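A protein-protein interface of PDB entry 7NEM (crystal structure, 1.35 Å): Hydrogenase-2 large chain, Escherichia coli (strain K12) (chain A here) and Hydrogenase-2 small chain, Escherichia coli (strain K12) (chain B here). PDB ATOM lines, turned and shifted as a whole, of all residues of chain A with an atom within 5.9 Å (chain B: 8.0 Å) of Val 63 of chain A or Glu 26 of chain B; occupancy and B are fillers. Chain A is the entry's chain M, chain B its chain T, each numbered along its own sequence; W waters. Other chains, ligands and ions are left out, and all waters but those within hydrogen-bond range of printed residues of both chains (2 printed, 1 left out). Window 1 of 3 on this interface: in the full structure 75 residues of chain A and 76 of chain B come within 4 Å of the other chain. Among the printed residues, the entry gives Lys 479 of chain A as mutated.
The side-chain sulfur (SG) of Cys 21 of chain B sits close to the backbone NH (N) of Gly 23 of chain B (3.3 Å).
NH1 of Arg 30 of chain B lies within salt-bridge range of OE1 of Glu 26 of chain B, at 2.9 Å.
OE1 of Glu 14 of chain A lies close to SG of Cys 546 of chain A, at 3.4 Å.
O of Val 63 of chain A sits close to NE2 of His 99 of chain A (3.3 Å).
OE1 of Gln 198 of chain A is in hydrogen-bond range of ND1 of His 102 of chain A, 2.8 Å away.
The backbone carbonyl oxygen of Val 106 of chain A sits at hydrogen-bond distance from the backbone NH of Leu 111 of chain A (3.0 Å).
Val 63 of chain A touches just these residues of chain B: Cys 21 (3.8 Å), Thr 22 (3.6 Å) and Glu 26 (3.5 Å).
Glu 26 of chain B touches four residues of chain A.
Gly 62 of chain A touches three residues of chain B.
Printed residues of chain A within 4 Å of Leu 29 of chain B: Val 106 (3.8 Å) and Gln 198 (3.0 Å).
Of the printed residues of chain B, Asn 202 of chain A touches Arg 30.
Of the printed residues of chain A, Thr 22 of chain B touches Glu 14 and Val 63.
Printed residues of chain A within 4 Å of Arg 30 of chain B: His 102 (3.6 Å), Asn 202 (3.1 Å) and Pro 213 (3.5 Å).
Printed residues of chain A within 4 Å of Val 51 of chain B: Leu 111 (3.3 Å).
Val 36 of chain B touches none of the printed residues of chain A.
His 99 of chain A touches none of the printed residues of chain B.
The nearest residue of chain B that does not touch Val 63 of chain A is Gly 23 of chain B (4.7 Å).
The backbone carbonyl oxygen (O) of Cys 21 of chain B is in hydrogen-bond range of the backbone NH (N) of Gly 62 of chain A (2.8 Å).
OG1 of Thr 22 of chain B sits at hydrogen-bond distance from OE2 of Glu 14 of chain A (2.5 Å).
NE2 of Gln 198 of chain A lies within hydrogen-bond range of O of Leu 29 of chain B.
NH2 of Arg 30 of chain B sits close to ND2 of Asn 202 of chain A (3.2 Å).
OE2 of Glu 14 of chain A lies close to O of Cys 21 of chain B (3.4 Å).
Of the 20 printed residues of chain B, 9 touch a printed residue of chain A.
Among the printed residues, no Asp or Glu carboxylate lies within 4 Å of a Lys or Arg side-chain nitrogen of the other chain.
Water W1 lies within hydrogen-bond range of the side-chain carboxylate of Glu 26 of chain B (2.6 Å) and a ring nitrogen (NE2) of His 102 of chain A (3.0 Å).
Water W2 lies within hydrogen-bond range of ND2 of Asn 202 of chain A (2.7 Å), OE1 of Gln 198 of chain A (2.9 Å) and O of Leu 29 of chain B (3.1 Å).
Among the printed residues, merely in contact across the chains: Leu 111 of chain A with Val 51 of chain B (3.3 Å), His 102 of chain A with Glu 26 of chain B (3.3 Å), Pro 213 of chain A with Pro 154 of chain B (3.4 Å), Pro 213 of chain A with Gly 23 of chain B (3.4 Å), Pro 213 of chain A with Arg 30 of chain B (3.5 Å), Gly 62 of chain A with Glu 26 of chain B (3.5 Å), Val 63 of chain A with Glu 26 of chain B (3.5 Å), Val 63 of chain A with Thr 22 of chain B (3.6 Å), His 102 of chain A with Arg 30 of chain B (3.6 Å), Gly 62 of chain A with Gly 23 of chain B (3.6 Å), Pro 213 of chain A with Glu 26 of chain B (3.7 Å), Cys 61 of chain A with Cys 21 of chain B (3.8 Å), Val 106 of chain A with Leu 29 of chain B (3.8 Å), Val 63 of chain A with Cys 21 of chain B (3.8 Å) and Pro 213 of chain A with Ser 27 of chain B (3.9 Å).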
ATOM      1  N   GLU A  14      26.818  12.794  -4.955  1.00  0.00           N
ATOM      2  CA  GLU A  14      26.469  14.212  -4.713  1.00  0.00           C
ATOM      3  C   GLU A  14      26.970  15.048  -5.886  1.00  0.00           C
ATOM      4  O   GLU A  14      28.153  14.935  -6.255  1.00  0.00           O
ATOM      5  CB  GLU A  14      27.056  14.691  -3.390  1.00  0.00           C
ATOM      6  CG  GLU A  14      26.548  16.074  -2.994  1.00  0.00           C
ATOM      7  CD  GLU A  14      26.903  17.227  -3.913  1.00  0.00           C
ATOM      8  OE1 GLU A  14      28.039  17.199  -4.441  1.00  0.00           O
ATOM      9  OE2 GLU A  14      26.053  18.176  -4.083  1.00  0.00           O
ATOM     10  N   CYS A  61      28.776  21.639   1.162  1.00  0.00           N
ATOM     11  CA  CYS A  61      28.144  20.323   0.924  1.00  0.00           C
ATOM     12  C   CYS A  61      27.156  19.963   2.029  1.00  0.00           C
ATOM     13  O   CYS A  61      27.490  20.112   3.219  1.00  0.00           O
ATOM     14  CB  CYS A  61      29.184  19.240   0.799  1.00  0.00           C
ATOM     15  SG  CYS A  61      28.483  17.667   0.302  1.00  0.00           S
ATOM     16  N   GLY A  62      25.996  19.492   1.628  1.00  0.00           N
ATOM     17  CA  GLY A  62      24.915  19.043   2.513  1.00  0.00           C
ATOM     18  C   GLY A  62      24.889  17.551   2.692  1.00  0.00           C
ATOM     19  O   GLY A  62      24.100  17.101   3.541  1.00  0.00           O
ATOM     20  N   VAL A  63      25.620  16.780   1.894  1.00  0.00           N
ATOM     21  CA  VAL A  63      25.781  15.345   2.153  1.00  0.00           C
ATOM     22  C   VAL A  63      26.822  15.220   3.258  1.00  0.00           C
ATOM     23  O   VAL A  63      26.439  14.756   4.339  1.00  0.00           O
ATOM     24  CB  VAL A  63      26.173  14.580   0.889  1.00  0.00           C
ATOM     25  CG1 VAL A  63      26.500  13.138   1.218  1.00  0.00           C
ATOM     26  CG2 VAL A  63      25.092  14.655  -0.191  1.00  0.00           C
ATOM     27  N   CYS A  64      28.041  15.726   3.051  1.00  0.00           N
ATOM     28  CA  CYS A  64      29.064  15.760   4.125  1.00  0.00           C
ATOM     29  C   CYS A  64      28.871  17.036   4.915  1.00  0.00           C
ATOM     30  O   CYS A  64      29.814  17.763   5.144  1.00  0.00           O
ATOM     31  CB  CYS A  64      30.464  15.538   3.589  1.00  0.00           C
ATOM     32  SG  CYS A  64      31.031  16.784   2.412  1.00  0.00           S
ATOM     33  N   THR A  65      27.633  17.264   5.341  1.00  0.00           N
ATOM     34  CA  THR A  65      27.353  18.333   6.309  1.00  0.00           C
ATOM     35  C   THR A  65      28.187  18.016   7.556  1.00  0.00           C
ATOM     36  O   THR A  65      28.729  16.893   7.702  1.00  0.00           O
ATOM     37  CB  THR A  65      25.847  18.449   6.511  1.00  0.00           C
ATOM     38  OG1 THR A  65      25.646  19.624   7.290  1.00  0.00           O
ATOM     39  CG2 THR A  65      25.254  17.257   7.216  1.00  0.00           C
ATOM     40  N   HIS A  99      27.607  11.575  12.197  1.00  0.00           N
ATOM     41  CA  HIS A  99      27.342  12.013  10.815  1.00  0.00           C
ATOM     42  C   HIS A  99      27.962  11.005   9.848  1.00  0.00           C
ATOM     43  O   HIS A  99      27.311  10.570   8.910  1.00  0.00           O
ATOM     44  CB  HIS A  99      27.938  13.401  10.524  1.00  0.00           C
ATOM     45  CG  HIS A  99      27.907  13.628   9.073  1.00  0.00           C
ATOM     46  ND1 HIS A  99      26.764  14.034   8.474  1.00  0.00           N
ATOM     47  CD2 HIS A  99      28.766  13.243   8.093  1.00  0.00           C
ATOM     48  CE1 HIS A  99      26.902  13.964   7.163  1.00  0.00           C
ATOM     49  NE2 HIS A  99      28.121  13.438   6.906  1.00  0.00           N
ATOM     50  N   HIS A 102      25.877   7.818   9.350  1.00  0.00           N
ATOM     51  CA  HIS A 102      24.799   8.110   8.373  1.00  0.00           C
ATOM     52  C   HIS A 102      25.392   8.085   6.967  1.00  0.00           C
ATOM     53  O   HIS A 102      24.799   7.493   6.065  1.00  0.00           O
ATOM     54  CB  HIS A 102      24.095   9.444   8.716  1.00  0.00           C
ATOM     55  CG  HIS A 102      23.669  10.246   7.543  1.00  0.00           C
ATOM     56  ND1 HIS A 102      22.465  10.073   6.884  1.00  0.00           N
ATOM     57  CD2 HIS A 102      24.312  11.254   6.930  1.00  0.00           C
ATOM     58  CE1 HIS A 102      22.443  10.975   5.891  1.00  0.00           C
ATOM     59  NE2 HIS A 102      23.569  11.666   5.883  1.00  0.00           N
ATOM     60  N   ASP A 103      26.480   8.769   6.783  1.00  0.00           N
ATOM     61  CA  ASP A 103      27.044   9.069   5.444  1.00  0.00           C
ATOM     62  C   ASP A 103      27.424   7.727   4.792  1.00  0.00           C
ATOM     63  O   ASP A 103      27.022   7.447   3.645  1.00  0.00           O
ATOM     64  CB  ASP A 103      28.212  10.046   5.660  1.00  0.00           C
ATOM     65  CG  ASP A 103      28.729  10.765   4.448  1.00  0.00           C
ATOM     66  OD1 ASP A 103      28.907  10.090   3.415  1.00  0.00           O
ATOM     67  OD2 ASP A 103      28.942  11.996   4.535  1.00  0.00           O
ATOM     68  N   VAL A 106      24.323   5.359   3.910  1.00  0.00           N
ATOM     69  CA  VAL A 106      23.563   5.848   2.738  1.00  0.00           C
ATOM     70  C   VAL A 106      24.404   5.596   1.487  1.00  0.00           C
ATOM     71  O   VAL A 106      23.830   5.219   0.426  1.00  0.00           O
ATOM     72  CB  VAL A 106      23.197   7.325   2.924  1.00  0.00           C
ATOM     73  CG1 VAL A 106      22.647   7.962   1.652  1.00  0.00           C
ATOM     74  CG2 VAL A 106      22.199   7.505   4.053  1.00  0.00           C
ATOM     75  N   LEU A 111      23.154   4.923  -2.496  1.00  0.00           N
ATOM     76  CA  LEU A 111      23.936   5.385  -3.659  1.00  0.00           C
ATOM     77  C   LEU A 111      24.542   4.217  -4.435  1.00  0.00           C
ATOM     78  O   LEU A 111      24.552   4.301  -5.661  1.00  0.00           O
ATOM     79  CB  LEU A 111      24.986   6.405  -3.243  1.00  0.00           C
ATOM     80  CG  LEU A 111      24.424   7.584  -2.449  1.00  0.00           C
ATOM     81  CD1 LEU A 111      25.512   8.577  -2.075  1.00  0.00           C
ATOM     82  CD2 LEU A 111      23.310   8.290  -3.190  1.00  0.00           C
ATOM     83  N   GLN A 198      20.250   5.062   9.493  1.00  0.00           N
ATOM     84  CA  GLN A 198      20.844   6.374   9.215  1.00  0.00           C
ATOM     85  C   GLN A 198      20.010   7.469   9.896  1.00  0.00           C
ATOM     86  O   GLN A 198      20.597   8.494  10.297  1.00  0.00           O
ATOM     87  CB  GLN A 198      21.060   6.579   7.714  1.00  0.00           C
ATOM     88  CG  GLN A 198      19.808   6.699   6.891  1.00  0.00           C
ATOM     89  CD  GLN A 198      19.168   8.066   6.891  1.00  0.00           C
ATOM     90  OE1 GLN A 198      19.855   9.101   6.968  1.00  0.00           O
ATOM     91  NE2 GLN A 198      17.854   8.052   6.688  1.00  0.00           N
ATOM     92  N   ASN A 202      21.426  10.382  12.571  1.00  0.00           N
ATOM     93  CA  ASN A 202      21.247  11.849  12.448  1.00  0.00           C
ATOM     94  C   ASN A 202      20.479  12.428  13.639  1.00  0.00           C
ATOM     95  O   ASN A 202      20.602  13.602  13.857  1.00  0.00           O
ATOM     96  CB  ASN A 202      20.672  12.228  11.100  1.00  0.00           C
ATOM     97  CG  ASN A 202      21.802  12.344  10.106  1.00  0.00           C
ATOM     98  OD1 ASN A 202      22.950  12.574  10.483  1.00  0.00           O
ATOM     99  ND2 ASN A 202      21.486  12.166   8.846  1.00  0.00           N
ATOM    100  N   PRO A 213      20.356  18.382   8.043  1.00  0.00           N
ATOM    101  CA  PRO A 213      21.637  18.960   7.642  1.00  0.00           C
ATOM    102  C   PRO A 213      21.957  20.374   8.136  1.00  0.00           C
ATOM    103  O   PRO A 213      21.057  21.162   8.493  1.00  0.00           O
ATOM    104  CB  PRO A 213      21.522  19.048   6.095  1.00  0.00           C
ATOM    105  CG  PRO A 213      20.462  18.084   5.738  1.00  0.00           C
ATOM    106  CD  PRO A 213      19.489  18.156   6.862  1.00  0.00           C
ATOM    107  N   LYS A 479      34.788  11.110   3.049  1.00  0.00           N
ATOM    108  CA  LYS A 479      35.435  10.883   1.727  1.00  0.00           C
ATOM    109  C   LYS A 479      36.952  11.004   1.815  1.00  0.00           C
ATOM    110  O   LYS A 479      37.617  10.728   0.790  1.00  0.00           O
ATOM    111  CB  LYS A 479      34.878  11.834   0.678  1.00  0.00           C
ATOM    112  CG  LYS A 479      33.723  11.295  -0.157  1.00  0.00           C
ATOM    113  CD  LYS A 479      32.340  11.818   0.178  1.00  0.00           C
ATOM    114  CE  LYS A 479      31.762  11.287   1.476  1.00  0.00           C
ATOM    115  NZ  LYS A 479      30.293  11.094   1.366  1.00  0.00           N
ATOM    116  N   ASP A 544      32.860   7.321  -3.768  1.00  0.00           N
ATOM    117  CA  ASP A 544      31.833   8.177  -3.110  1.00  0.00           C
ATOM    118  C   ASP A 544      31.989   9.611  -3.580  1.00  0.00           C
ATOM    119  O   ASP A 544      32.226  10.563  -2.818  1.00  0.00           O
ATOM    120  CB  ASP A 544      32.008   8.039  -1.612  1.00  0.00           C
ATOM    121  CG  ASP A 544      30.908   8.600  -0.737  1.00  0.00           C
ATOM    122  OD1 ASP A 544      29.899   9.116  -1.258  1.00  0.00           O
ATOM    123  OD2 ASP A 544      31.118   8.500   0.486  1.00  0.00           O
ATOM    124  N   CYS A 546      31.728  13.414  -4.443  1.00  0.00           N
ATOM    125  CA  CYS A 546      30.971  14.585  -3.994  1.00  0.00           C
ATOM    126  C   CYS A 546      31.513  15.788  -4.731  1.00  0.00           C
ATOM    127  O   CYS A 546      32.620  16.252  -4.455  1.00  0.00           O
ATOM    128  CB  CYS A 546      31.103  14.754  -2.502  1.00  0.00           C
ATOM    129  SG  CYS A 546      30.104  16.143  -1.919  1.00  0.00           S
ATOM    130  N   TRP B  15      12.507  16.452  -9.967  1.00  0.00           N
ATOM    131  CA  TRP B  15      13.450  17.206  -9.096  1.00  0.00           C
ATOM    132  C   TRP B  15      14.747  17.485  -9.844  1.00  0.00           C
ATOM    133  O   TRP B  15      15.413  16.520 -10.250  1.00  0.00           O
ATOM    134  CB  TRP B  15      13.691  16.427  -7.812  1.00  0.00           C
ATOM    135  CG  TRP B  15      14.459  17.159  -6.758  1.00  0.00           C
ATOM    136  CD1 TRP B  15      15.709  17.711  -6.844  1.00  0.00           C
ATOM    137  CD2 TRP B  15      14.072  17.285  -5.368  1.00  0.00           C
ATOM    138  NE1 TRP B  15      16.107  18.220  -5.633  1.00  0.00           N
ATOM    139  CE2 TRP B  15      15.113  17.996  -4.726  1.00  0.00           C
ATOM    140  CE3 TRP B  15      12.955  16.880  -4.650  1.00  0.00           C
ATOM    141  CZ2 TRP B  15      15.059  18.283  -3.360  1.00  0.00           C
ATOM    142  CZ3 TRP B  15      12.889  17.175  -3.308  1.00  0.00           C
ATOM    143  CH2 TRP B  15      13.936  17.860  -2.690  1.00  0.00           C
ATOM    144  N   CYS B  21      23.824  22.137  -2.821  1.00  0.00           N
ATOM    145  CA  CYS B  21      24.821  21.422  -1.977  1.00  0.00           C
ATOM    146  C   CYS B  21      24.313  20.027  -1.610  1.00  0.00           C
ATOM    147  O   CYS B  21      25.037  19.241  -0.989  1.00  0.00           O
ATOM    148  CB  CYS B  21      25.141  22.216  -0.713  1.00  0.00           C
ATOM    149  SG  CYS B  21      23.885  22.057   0.605  1.00  0.00           S
ATOM    150  N   THR B  22      23.066  19.729  -1.967  1.00  0.00           N
ATOM    151  CA  THR B  22      22.366  18.443  -1.746  1.00  0.00           C
ATOM    152  C   THR B  22      21.722  18.427  -0.347  1.00  0.00           C
ATOM    153  O   THR B  22      20.982  17.484  -0.036  1.00  0.00           O
ATOM    154  CB  THR B  22      23.192  17.198  -2.072  1.00  0.00           C
ATOM    155  OG1 THR B  22      23.778  17.491  -3.354  1.00  0.00           O
ATOM    156  CG2 THR B  22      22.397  15.920  -2.168  1.00  0.00           C
ATOM    157  N   GLY B  23      21.963  19.430   0.493  1.00  0.00           N
ATOM    158  CA  GLY B  23      21.331  19.488   1.803  1.00  0.00           C
ATOM    159  C   GLY B  23      19.824  19.454   1.751  1.00  0.00           C
ATOM    160  O   GLY B  23      19.184  18.934   2.694  1.00  0.00           O
ATOM    161  N   CYS B  24      19.223  20.064   0.724  1.00  0.00           N
ATOM    162  CA  CYS B  24      17.745  20.107   0.607  1.00  0.00           C
ATOM    163  C   CYS B  24      17.187  18.718   0.294  1.00  0.00           C
ATOM    164  O   CYS B  24      16.184  18.308   0.904  1.00  0.00           O
ATOM    165  CB  CYS B  24      17.347  21.160  -0.429  1.00  0.00           C
ATOM    166  SG  CYS B  24      17.538  22.854   0.190  1.00  0.00           S
ATOM    167  N   THR B  25      17.834  17.921  -0.545  1.00  0.00           N
ATOM    168  CA  THR B  25      17.459  16.501  -0.718  1.00  0.00           C
ATOM    169  C   THR B  25      17.737  15.721   0.580  1.00  0.00           C
ATOM    170  O   THR B  25      16.862  14.914   1.030  1.00  0.00           O
ATOM    171  CB  THR B  25      18.257  15.863  -1.843  1.00  0.00           C
ATOM    172  OG1 THR B  25      17.769  16.424  -3.073  1.00  0.00           O
ATOM    173  CG2 THR B  25      18.111  14.366  -1.851  1.00  0.00           C
ATOM    174  N   GLU B  26      18.893  15.976   1.214  1.00  0.00           N
ATOM    175  CA  GLU B  26      19.249  15.234   2.461  1.00  0.00           C
ATOM    176  C   GLU B  26      18.218  15.469   3.557  1.00  0.00           C
ATOM    177  O   GLU B  26      18.040  14.575   4.401  1.00  0.00           O
ATOM    178  CB  GLU B  26      20.634  15.622   2.959  1.00  0.00           C
ATOM    179  CG  GLU B  26      21.749  14.952   2.159  1.00  0.00           C
ATOM    180  CD  GLU B  26      22.006  13.517   2.550  1.00  0.00           C
ATOM    181  OE1 GLU B  26      21.346  12.972   3.446  1.00  0.00           O
ATOM    182  OE2 GLU B  26      22.838  12.886   1.846  1.00  0.00           O
ATOM    183  N   SER B  27      17.563  16.624   3.566  1.00  0.00           N
ATOM    184  CA  SER B  27      16.526  16.871   4.586  1.00  0.00           C
ATOM    185  C   SER B  27      15.480  15.761   4.517  1.00  0.00           C
ATOM    186  O   SER B  27      14.934  15.352   5.574  1.00  0.00           O
ATOM    187  CB  SER B  27      15.900  18.239   4.411  1.00  0.00           C
ATOM    188  OG  SER B  27      14.974  18.274   3.339  1.00  0.00           O
ATOM    189  N   LEU B  28      15.177  15.219   3.321  1.00  0.00           N
ATOM    190  CA  LEU B  28      14.146  14.163   3.198  1.00  0.00           C
ATOM    191  C   LEU B  28      14.557  12.923   3.984  1.00  0.00           C
ATOM    192  O   LEU B  28      13.671  12.189   4.416  1.00  0.00           O
ATOM    193  CB  LEU B  28      13.904  13.764   1.740  1.00  0.00           C
ATOM    194  CG  LEU B  28      13.478  14.914   0.844  1.00  0.00           C
ATOM    195  CD1 LEU B  28      13.346  14.429  -0.595  1.00  0.00           C
ATOM    196  CD2 LEU B  28      12.172  15.518   1.336  1.00  0.00           C
ATOM    197  N   LEU B  29      15.854  12.689   4.171  1.00  0.00           N
ATOM    198  CA  LEU B  29      16.327  11.480   4.876  1.00  0.00           C
ATOM    199  C   LEU B  29      16.114  11.608   6.395  1.00  0.00           C
ATOM    200  O   LEU B  29      16.300  10.600   7.069  1.00  0.00           O
ATOM    201  CB  LEU B  29      17.784  11.192   4.512  1.00  0.00           C
ATOM    202  CG  LEU B  29      17.971  10.287   3.280  1.00  0.00           C
ATOM    203  CD1 LEU B  29      17.415  10.908   2.001  1.00  0.00           C
ATOM    204  CD2 LEU B  29      19.421   9.934   3.082  1.00  0.00           C
ATOM    205  N   ARG B  30      15.747  12.780   6.904  1.00  0.00           N
ATOM    206  CA  ARG B  30      15.413  12.981   8.327  1.00  0.00           C
ATOM    207  C   ARG B  30      13.890  12.954   8.506  1.00  0.00           C
ATOM    208  O   ARG B  30      13.419  12.886   9.671  1.00  0.00           O
ATOM    209  CB  ARG B  30      15.943  14.321   8.847  1.00  0.00           C
ATOM    210  CG  ARG B  30      17.445  14.431   9.043  1.00  0.00           C
ATOM    211  CD  ARG B  30      18.198  14.477   7.745  1.00  0.00           C
ATOM    212  NE  ARG B  30      19.584  14.871   7.925  1.00  0.00           N
ATOM    213  CZ  ARG B  30      20.594  14.620   7.120  1.00  0.00           C
ATOM    214  NH1 ARG B  30      20.408  13.927   6.003  1.00  0.00           N
ATOM    215  NH2 ARG B  30      21.811  15.065   7.416  1.00  0.00           N
ATOM    216  N   ALA B  31      13.117  13.061   7.433  1.00  0.00           N
ATOM    217  CA  ALA B  31      11.663  13.171   7.545  1.00  0.00           C
ATOM    218  C   ALA B  31      11.042  11.908   8.151  1.00  0.00           C
ATOM    219  O   ALA B  31      11.558  10.789   7.939  1.00  0.00           O
ATOM    220  CB  ALA B  31      11.029  13.459   6.204  1.00  0.00           C
ATOM    221  N   VAL B  36      11.294   9.086   3.770  1.00  0.00           N
ATOM    222  CA  VAL B  36      11.645   9.167   2.326  1.00  0.00           C
ATOM    223  C   VAL B  36      11.199   7.887   1.612  1.00  0.00           C
ATOM    224  O   VAL B  36      10.732   8.001   0.442  1.00  0.00           O
ATOM    225  CB  VAL B  36      13.128   9.468   2.146  1.00  0.00           C
ATOM    226  CG1 VAL B  36      14.037   8.388   2.690  1.00  0.00           C
ATOM    227  CG2 VAL B  36      13.403   9.788   0.679  1.00  0.00           C
ATOM    228  N   HIS B  49      15.239  12.252 -10.135  1.00  0.00           N
ATOM    229  CA  HIS B  49      16.042  12.699  -8.966  1.00  0.00           C
ATOM    230  C   HIS B  49      17.397  12.009  -9.081  1.00  0.00           C
ATOM    231  O   HIS B  49      17.492  10.815  -8.834  1.00  0.00           O
ATOM    232  CB  HIS B  49      15.370  12.388  -7.603  1.00  0.00           C
ATOM    233  CG  HIS B  49      15.963  13.293  -6.593  1.00  0.00           C
ATOM    234  ND1 HIS B  49      17.339  13.358  -6.401  1.00  0.00           N
ATOM    235  CD2 HIS B  49      15.388  14.120  -5.686  1.00  0.00           C
ATOM    236  CE1 HIS B  49      17.562  14.320  -5.484  1.00  0.00           C
ATOM    237  NE2 HIS B  49      16.399  14.754  -5.004  1.00  0.00           N
ATOM    238  N   VAL B  51      20.012  12.026  -7.342  1.00  0.00           N
ATOM    239  CA  VAL B  51      20.697  11.461  -6.146  1.00  0.00           C
ATOM    240  C   VAL B  51      20.318   9.993  -5.981  1.00  0.00           C
ATOM    241  O   VAL B  51      21.144   9.235  -5.503  1.00  0.00           O
ATOM    242  CB  VAL B  51      20.417  12.294  -4.873  1.00  0.00           C
ATOM    243  CG1 VAL B  51      20.986  11.602  -3.626  1.00  0.00           C
ATOM    244  CG2 VAL B  51      20.966  13.697  -4.987  1.00  0.00           C
ATOM    245  N   ASP B  80      16.298  22.612  -6.205  1.00  0.00           N
ATOM    246  CA  ASP B  80      17.224  23.117  -5.158  1.00  0.00           C
ATOM    247  C   ASP B  80      18.449  23.720  -5.828  1.00  0.00           C
ATOM    248  O   ASP B  80      18.860  23.303  -6.937  1.00  0.00           O
ATOM    249  CB  ASP B  80      17.593  22.067  -4.104  1.00  0.00           C
ATOM    250  CG  ASP B  80      18.153  20.755  -4.615  1.00  0.00           C
ATOM    251  OD1 ASP B  80      18.010  20.424  -5.827  1.00  0.00           O
ATOM    252  OD2 ASP B  80      18.768  20.008  -3.793  1.00  0.00           O
ATOM    253  N   ILE B 116      12.713  24.669  -3.290  1.00  0.00           N
ATOM    254  CA  ILE B 116      13.064  24.144  -1.934  1.00  0.00           C
ATOM    255  C   ILE B 116      14.443  24.711  -1.552  1.00  0.00           C
ATOM    256  O   ILE B 116      15.407  24.501  -2.321  1.00  0.00           O
ATOM    257  CB  ILE B 116      12.944  22.625  -1.855  1.00  0.00           C
ATOM    258  CG1 ILE B 116      13.074  22.231  -0.386  1.00  0.00           C
ATOM    259  CG2 ILE B 116      13.948  21.900  -2.680  1.00  0.00           C
ATOM    260  CD1 ILE B 116      12.997  20.732  -0.137  1.00  0.00           C
ATOM    261  N   PRO B 154      19.001  23.675   5.226  1.00  0.00           N
ATOM    262  CA  PRO B 154      17.761  23.500   4.466  1.00  0.00           C
ATOM    263  C   PRO B 154      16.559  23.681   5.380  1.00  0.00           C
ATOM    264  O   PRO B 154      16.648  23.625   6.618  1.00  0.00           O
ATOM    265  CB  PRO B 154      17.847  22.048   4.010  1.00  0.00           C
ATOM    266  CG  PRO B 154      18.548  21.375   5.179  1.00  0.00           C
ATOM    267  CD  PRO B 154      19.521  22.396   5.725  1.00  0.00           C
ATOM    268  N   PRO B 155      15.335  23.842   4.809  1.00  0.00           N
ATOM    269  CA  PRO B 155      14.134  23.857   5.630  1.00  0.00           C
ATOM    270  C   PRO B 155      13.932  22.507   6.308  1.00  0.00           C
ATOM    271  O   PRO B 155      14.379  21.465   5.837  1.00  0.00           O
ATOM    272  CB  PRO B 155      13.020  24.050   4.581  1.00  0.00           C
ATOM    273  CG  PRO B 155      13.589  23.442   3.350  1.00  0.00           C
ATOM    274  CD  PRO B 155      15.042  23.831   3.364  1.00  0.00           C
ATOM    275  N   PRO B 157      12.131  19.332   6.441  1.00  0.00           N
ATOM    276  CA  PRO B 157      11.624  18.680   5.234  1.00  0.00           C
ATOM    277  C   PRO B 157      10.103  18.708   5.185  1.00  0.00           C
ATOM    278  O   PRO B 157       9.530  18.672   4.082  1.00  0.00           O
ATOM    279  CB  PRO B 157      12.173  17.253   5.293  1.00  0.00           C
ATOM    280  CG  PRO B 157      12.439  17.059   6.760  1.00  0.00           C
ATOM    281  CD  PRO B 157      12.950  18.391   7.256  1.00  0.00           C
HETATM  282  O   HOH W   1      23.978  10.840   2.986  1.00  0.00           O
HETATM  283  O   HOH W   2      18.921  11.307   8.609  1.00  0.00           O
